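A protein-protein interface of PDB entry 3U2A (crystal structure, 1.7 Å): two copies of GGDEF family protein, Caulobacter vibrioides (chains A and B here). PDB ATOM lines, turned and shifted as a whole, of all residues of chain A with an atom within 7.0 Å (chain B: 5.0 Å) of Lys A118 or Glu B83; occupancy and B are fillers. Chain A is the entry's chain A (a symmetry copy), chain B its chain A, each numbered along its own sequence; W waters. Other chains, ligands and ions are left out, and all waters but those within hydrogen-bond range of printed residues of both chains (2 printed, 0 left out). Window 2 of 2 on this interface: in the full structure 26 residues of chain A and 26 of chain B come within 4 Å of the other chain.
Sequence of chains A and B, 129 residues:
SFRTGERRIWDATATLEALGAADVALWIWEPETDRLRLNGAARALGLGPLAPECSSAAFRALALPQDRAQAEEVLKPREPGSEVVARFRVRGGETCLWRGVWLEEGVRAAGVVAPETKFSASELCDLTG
Ser B120 touches its own counterpart, Ser A120.
The side-chain amino group of Lys A118 is in salt-bridge range of the side-chain carboxylate of Glu B83, 3.97 Å away.
The backbone NH of Ser A120 lies within hydrogen-bond range of the backbone carbonyl oxygen of Ser B120 (3.4 Å).
NH2 of Arg B99 lies within salt-bridge range of OE1 of Glu B83 (3.8 Å).
The backbone NH of Val B84 is in hydrogen-bond range of the backbone carbonyl oxygen of Gly B100 (2.9 Å).
Water W2 lies within hydrogen-bond range of O of Ser B120 and O of Lys A118.
Water W1 lies within hydrogen-bond range of the side-chain amino group of Lys A118 (2.7 Å), the backbone carbonyl oxygen of Ala A21 (3.1 Å) and the backbone carbonyl oxygen of Gly B100 (3.4 Å).
Ala A21 touches Gly B100 (O to C, 3.9 Å).
CB of Ala A21 touches CG1 of Val B101, 3.7 Å away.
Ala A22 touches Arg B99 (CB to O, 3.8 Å).
Lys A118 touches Arg B99.
Lys A118 touches Ser B120 (O to O, 3.6 Å).
CZ of Phe A119 touches CB of Arg B99 (3.7 Å).
O of Ser B120 touches CA of Phe A119, at 3.7 Å.
Printed residues of chain B within 4 Å of Ala A21: Gly B100 and Val B101.
Lys A118 touches just these residues of chain B: Glu B83, Arg B99 and Ser B120.
Glu B83 touches just one residue of chain A: Lys A118.
Of the printed residues of chain A, Ser B120 touches Lys A118 (3.6 Å), Phe A119 (3.7 Å) and Ser A120 (3.4 Å).
The nearest residue of chain B that does not touch Lys A118 is Leu B97 (4.9 Å).
The nearest printed residue of chain B that does not touch Ser A120 is Leu B97 (6.4 Å).
Of the 13 printed residues of chain A, 5 touch a printed residue of chain B.
Hydrophobic or aromatic side chains of chain A that line the printed part of chain B: Ala A21, Ala A22 and Phe A119.
Printed residues of chain B that touch a printed residue of chain A: Glu B83, Arg B99, Gly B100, Val B101 and Ser B120.
Hydrophobic or aromatic side chains of chain B that line the printed part of chain A: Val B101.
Among the printed residues, 9 pairs touch across the chains.
Among the printed residues, Asp or Glu carboxylates within 4 Å of a Lys or Arg side-chain nitrogen of the other chain: Lys A118 with Glu B83.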
ATOM      1  N   GLY A  20      -0.624  30.661  13.258  1.00  0.00           N
ATOM      2  CA  GLY A  20       0.326  31.599  13.852  1.00  0.00           C
ATOM      3  C   GLY A  20       1.415  30.894  14.638  1.00  0.00           C
ATOM      4  O   GLY A  20       2.586  31.269  14.563  1.00  0.00           O
ATOM      5  N   ALA A  21       1.022  29.865  15.387  1.00  0.00           N
ATOM      6  CA  ALA A  21       1.940  29.099  16.228  1.00  0.00           C
ATOM      7  C   ALA A  21       2.961  28.341  15.382  1.00  0.00           C
ATOM      8  O   ALA A  21       4.138  28.272  15.727  1.00  0.00           O
ATOM      9  CB  ALA A  21       1.167  28.141  17.106  1.00  0.00           C
ATOM     10  N   ALA A  22       2.488  27.788  14.265  1.00  0.00           N
ATOM     11  CA  ALA A  22       3.328  27.065  13.321  1.00  0.00           C
ATOM     12  C   ALA A  22       4.143  27.995  12.414  1.00  0.00           C
ATOM     13  O   ALA A  22       5.118  27.558  11.810  1.00  0.00           O
ATOM     14  CB  ALA A  22       2.469  26.133  12.495  1.00  0.00           C
ATOM     15  N   ASP A  23       3.753  29.273  12.345  1.00  0.00           N
ATOM     16  CA  ASP A  23       4.351  30.267  11.435  1.00  0.00           C
ATOM     17  C   ASP A  23       4.101  29.888   9.977  1.00  0.00           C
ATOM     18  O   ASP A  23       5.005  29.929   9.149  1.00  0.00           O
ATOM     19  CB  ASP A  23       5.851  30.431  11.693  1.00  0.00           C
ATOM     20  CG  ASP A  23       6.393  31.746  11.167  1.00  0.00           C
ATOM     21  OD1 ASP A  23       5.615  32.724  11.127  1.00  0.00           O
ATOM     22  OD2 ASP A  23       7.594  31.801  10.798  1.00  0.00           O
ATOM     23  N   VAL A  24       2.860  29.505   9.694  1.00  0.00           N
ATOM     24  CA  VAL A  24       2.431  28.992   8.390  1.00  0.00           C
ATOM     25  C   VAL A  24       1.228  29.823   7.897  1.00  0.00           C
ATOM     26  O   VAL A  24       0.490  30.397   8.717  1.00  0.00           O
ATOM     27  CB  VAL A  24       2.065  27.470   8.545  1.00  0.00           C
ATOM     28  CG1 VAL A  24       1.053  26.973   7.496  1.00  0.00           C
ATOM     29  CG2 VAL A  24       3.325  26.611   8.556  1.00  0.00           C
ATOM     30  N   LEU A  45       5.683  35.884   7.430  1.00  0.00           N
ATOM     31  CA  LEU A  45       6.387  35.247   6.328  1.00  0.00           C
ATOM     32  C   LEU A  45       6.874  36.219   5.248  1.00  0.00           C
ATOM     33  O   LEU A  45       7.498  35.797   4.267  1.00  0.00           O
ATOM     34  CB  LEU A  45       5.505  34.167   5.697  1.00  0.00           C
ATOM     35  CG  LEU A  45       5.239  32.941   6.563  1.00  0.00           C
ATOM     36  CD1 LEU A  45       4.258  32.040   5.871  1.00  0.00           C
ATOM     37  CD2 LEU A  45       6.518  32.209   6.846  1.00  0.00           C
ATOM     38  N   ALA A 114       5.127  27.908   4.066  1.00  0.00           N
ATOM     39  CA  ALA A 114       5.867  27.730   5.303  1.00  0.00           C
ATOM     40  C   ALA A 114       7.259  28.305   5.176  1.00  0.00           C
ATOM     41  O   ALA A 114       7.808  28.343   4.082  1.00  0.00           O
ATOM     42  CB  ALA A 114       5.938  26.258   5.646  1.00  0.00           C
ATOM     43  N   PRO A 115       7.847  28.741   6.300  1.00  0.00           N
ATOM     44  CA  PRO A 115       9.232  29.224   6.231  1.00  0.00           C
ATOM     45  C   PRO A 115      10.182  28.053   6.118  1.00  0.00           C
ATOM     46  O   PRO A 115      10.032  27.061   6.832  1.00  0.00           O
ATOM     47  CB  PRO A 115       9.433  29.948   7.565  1.00  0.00           C
ATOM     48  CG  PRO A 115       8.360  29.494   8.448  1.00  0.00           C
ATOM     49  CD  PRO A 115       7.315  28.752   7.672  1.00  0.00           C
ATOM     50  N   GLU A 116      11.155  28.130   5.218  1.00  0.00           N
ATOM     51  CA  GLU A 116      12.044  26.980   5.065  1.00  0.00           C
ATOM     52  C   GLU A 116      13.037  26.836   6.241  1.00  0.00           C
ATOM     53  O   GLU A 116      13.647  25.776   6.432  1.00  0.00           O
ATOM     54  CB  GLU A 116      12.694  26.937   3.676  1.00  0.00           C
ATOM     55  CG  GLU A 116      13.990  27.661   3.553  1.00  0.00           C
ATOM     56  CD  GLU A 116      14.839  27.126   2.419  1.00  0.00           C
ATOM     57  OE1 GLU A 116      14.294  26.423   1.534  1.00  0.00           O
ATOM     58  OE2 GLU A 116      16.054  27.414   2.418  1.00  0.00           O
ATOM     59  N   THR A 117      13.146  27.896   7.045  1.00  0.00           N
ATOM     60  CA  THR A 117      13.905  27.877   8.293  1.00  0.00           C
ATOM     61  C   THR A 117      13.326  26.872   9.304  1.00  0.00           C
ATOM     62  O   THR A 117      13.970  26.541  10.304  1.00  0.00           O
ATOM     63  CB  THR A 117      14.023  29.306   8.905  1.00  0.00           C
ATOM     64  OG1 THR A 117      15.084  29.335   9.867  1.00  0.00           O
ATOM     65  CG2 THR A 117      12.710  29.770   9.557  1.00  0.00           C
ATOM     66  N   LYS A 118      12.117  26.382   9.020  1.00  0.00           N
ATOM     67  CA  LYS A 118      11.402  25.437   9.886  1.00  0.00           C
ATOM     68  C   LYS A 118      10.912  24.208   9.110  1.00  0.00           C
ATOM     69  O   LYS A 118      10.872  23.098   9.652  1.00  0.00           O
ATOM     70  CB  LYS A 118      10.217  26.129  10.564  1.00  0.00           C
ATOM     71  CG  LYS A 118      10.593  27.306  11.466  1.00  0.00           C
ATOM     72  CD  LYS A 118       9.450  28.302  11.598  1.00  0.00           C
ATOM     73  CE  LYS A 118       8.371  27.812  12.553  1.00  0.00           C
ATOM     74  NZ  LYS A 118       8.596  28.347  13.926  1.00  0.00           N
ATOM     75  N   PHE A 119      10.544  24.413   7.845  1.00  0.00           N
ATOM     76  CA  PHE A 119       9.998  23.351   6.996  1.00  0.00           C
ATOM     77  C   PHE A 119      10.791  23.230   5.690  1.00  0.00           C
ATOM     78  O   PHE A 119      11.214  24.241   5.124  1.00  0.00           O
ATOM     79  CB  PHE A 119       8.520  23.625   6.690  1.00  0.00           C
ATOM     80  CG  PHE A 119       7.655  23.796   7.920  1.00  0.00           C
ATOM     81  CD1 PHE A 119       6.931  22.719   8.433  1.00  0.00           C
ATOM     82  CD2 PHE A 119       7.552  25.036   8.555  1.00  0.00           C
ATOM     83  CE1 PHE A 119       6.127  22.873   9.561  1.00  0.00           C
ATOM     84  CE2 PHE A 119       6.756  25.199   9.686  1.00  0.00           C
ATOM     85  CZ  PHE A 119       6.038  24.118  10.190  1.00  0.00           C
ATOM     86  N   SER A 120      10.984  21.996   5.214  1.00  0.00           N
ATOM     87  CA  SER A 120      11.770  21.729   3.993  1.00  0.00           C
ATOM     88  C   SER A 120      11.002  20.937   2.932  1.00  0.00           C
ATOM     89  O   SER A 120      10.524  19.836   3.188  1.00  0.00           O
ATOM     90  CB  SER A 120      13.083  21.021   4.329  1.00  0.00           C
ATOM     91  OG  SER A 120      13.972  21.899   4.992  1.00  0.00           O
ATOM     92  N   ARG B  78       5.075  23.334  28.526  1.00  0.00           N
ATOM     93  CA  ARG B  78       6.259  24.176  28.464  1.00  0.00           C
ATOM     94  C   ARG B  78       5.837  25.616  28.703  1.00  0.00           C
ATOM     95  O   ARG B  78       4.648  25.958  28.608  1.00  0.00           O
ATOM     96  CB  ARG B  78       6.953  24.067  27.097  1.00  0.00           C
ATOM     97  CG  ARG B  78       7.414  22.655  26.698  1.00  0.00           C
ATOM     98  CD  ARG B  78       7.957  22.588  25.280  1.00  0.00           C
ATOM     99  NE  ARG B  78       7.866  21.210  24.770  1.00  0.00           N
ATOM    100  CZ  ARG B  78       8.807  20.278  24.912  1.00  0.00           C
ATOM    101  NH1 ARG B  78       9.960  20.554  25.525  1.00  0.00           N
ATOM    102  NH2 ARG B  78       8.597  19.057  24.423  1.00  0.00           N
ATOM    103  N   GLY B  81       5.990  30.516  24.564  1.00  0.00           N
ATOM    104  CA  GLY B  81       7.051  30.777  23.608  1.00  0.00           C
ATOM    105  C   GLY B  81       7.932  29.583  23.285  1.00  0.00           C
ATOM    106  O   GLY B  81       8.696  29.631  22.316  1.00  0.00           O
ATOM    107  N   SER B  82       7.827  28.510  24.077  1.00  0.00           N
ATOM    108  CA  SER B  82       8.612  27.293  23.845  1.00  0.00           C
ATOM    109  C   SER B  82       8.174  26.578  22.561  1.00  0.00           C
ATOM    110  O   SER B  82       6.989  26.292  22.374  1.00  0.00           O
ATOM    111  CB  SER B  82       8.495  26.323  25.028  1.00  0.00           C
ATOM    112  OG  SER B  82       9.073  26.874  26.203  1.00  0.00           O
ATOM    113  N   GLU B  83       9.134  26.305  21.680  1.00  0.00           N
ATOM    114  CA  GLU B  83       8.849  25.572  20.447  1.00  0.00           C
ATOM    115  C   GLU B  83       8.450  24.135  20.748  1.00  0.00           C
ATOM    116  O   GLU B  83       8.965  23.526  21.693  1.00  0.00           O
ATOM    117  CB  GLU B  83      10.062  25.580  19.531  1.00  0.00           C
ATOM    118  CG  GLU B  83      10.174  26.830  18.661  1.00  0.00           C
ATOM    119  CD  GLU B  83      11.185  26.668  17.525  1.00  0.00           C
ATOM    120  OE1 GLU B  83      11.840  25.600  17.431  1.00  0.00           O
ATOM    121  OE2 GLU B  83      11.322  27.616  16.721  1.00  0.00           O
ATOM    122  N   VAL B  84       7.499  23.626  19.967  1.00  0.00           N
ATOM    123  CA  VAL B  84       7.147  22.213  19.955  1.00  0.00           C
ATOM    124  C   VAL B  84       7.632  21.648  18.626  1.00  0.00           C
ATOM    125  O   VAL B  84       7.233  22.125  17.556  1.00  0.00           O
ATOM    126  CB  VAL B  84       5.625  22.007  20.091  1.00  0.00           C
ATOM    127  CG1 VAL B  84       5.256  20.530  19.954  1.00  0.00           C
ATOM    128  CG2 VAL B  84       5.122  22.553  21.422  1.00  0.00           C
ATOM    129  N   VAL B  85       8.521  20.657  18.694  1.00  0.00           N
ATOM    130  CA  VAL B  85       8.999  19.941  17.508  1.00  0.00           C
ATOM    131  C   VAL B  85       9.036  18.451  17.845  1.00  0.00           C
ATOM    132  O   VAL B  85       9.701  18.024  18.798  1.00  0.00           O
ATOM    133  CB  VAL B  85      10.405  20.424  17.021  1.00  0.00           C
ATOM    134  CG1 VAL B  85      10.831  19.665  15.761  1.00  0.00           C
ATOM    135  CG2 VAL B  85      10.407  21.915  16.741  1.00  0.00           C
ATOM    136  N   LEU B  97       5.506  15.087  11.162  1.00  0.00           N
ATOM    137  CA  LEU B  97       6.181  16.131  11.882  1.00  0.00           C
ATOM    138  C   LEU B  97       5.141  17.064  12.506  1.00  0.00           C
ATOM    139  O   LEU B  97       4.251  17.586  11.826  1.00  0.00           O
ATOM    140  CB  LEU B  97       7.087  16.900  10.923  1.00  0.00           C
ATOM    141  CG  LEU B  97       7.667  18.234  11.393  1.00  0.00           C
ATOM    142  CD1 LEU B  97       8.808  18.035  12.423  1.00  0.00           C
ATOM    143  CD2 LEU B  97       8.131  19.040  10.173  1.00  0.00           C
ATOM    144  N   ARG B  99       4.858  20.629  14.481  1.00  0.00           N
ATOM    145  CA  ARG B  99       5.571  21.879  14.757  1.00  0.00           C
ATOM    146  C   ARG B  99       4.607  22.927  15.297  1.00  0.00           C
ATOM    147  O   ARG B  99       3.572  23.214  14.701  1.00  0.00           O
ATOM    148  CB  ARG B  99       6.230  22.429  13.490  1.00  0.00           C
ATOM    149  CG  ARG B  99       7.293  21.537  12.863  1.00  0.00           C
ATOM    150  CD  ARG B  99       8.737  21.874  13.272  1.00  0.00           C
ATOM    151  NE  ARG B  99       8.948  23.266  13.686  1.00  0.00           N
ATOM    152  CZ  ARG B  99      10.122  23.901  13.651  1.00  0.00           C
ATOM    153  NH1 ARG B  99      11.214  23.299  13.182  1.00  0.00           N
ATOM    154  NH2 ARG B  99      10.206  25.157  14.074  1.00  0.00           N
ATOM    155  N   GLY B 100       4.954  23.534  16.423  1.00  0.00           N
ATOM    156  CA  GLY B 100       4.113  24.598  16.969  1.00  0.00           C
ATOM    157  C   GLY B 100       4.814  25.310  18.105  1.00  0.00           C
ATOM    158  O   GLY B 100       6.048  25.346  18.156  1.00  0.00           O
ATOM    159  N   VAL B 101       4.023  25.889  19.002  1.00  0.00           N
ATOM    160  CA  VAL B 101       4.582  26.669  20.105  1.00  0.00           C
ATOM    161  C   VAL B 101       3.585  26.699  21.254  1.00  0.00           C
ATOM    162  O   VAL B 101       2.377  26.543  21.035  1.00  0.00           O
ATOM    163  CB  VAL B 101       4.934  28.138  19.633  1.00  0.00           C
ATOM    164  CG1 VAL B 101       3.724  29.018  19.641  1.00  0.00           C
ATOM    165  CG2 VAL B 101       6.009  28.761  20.507  1.00  0.00           C
ATOM    166  N   SER B 120       9.755  18.349   6.102  1.00  0.00           N
ATOM    167  CA  SER B 120      10.859  17.893   6.969  1.00  0.00           C
ATOM    168  C   SER B 120      11.175  18.857   8.114  1.00  0.00           C
ATOM    169  O   SER B 120      11.476  20.026   7.892  1.00  0.00           O
ATOM    170  CB  SER B 120      12.121  17.615   6.152  1.00  0.00           C
ATOM    171  OG  SER B 120      11.959  16.460   5.352  1.00  0.00           O
HETATM  172  O   HOH W   1       6.821  26.764  15.168  1.00  0.00           O
HETATM  173  O   HOH W   2      13.541  21.351   8.762  1.00  0.00           O
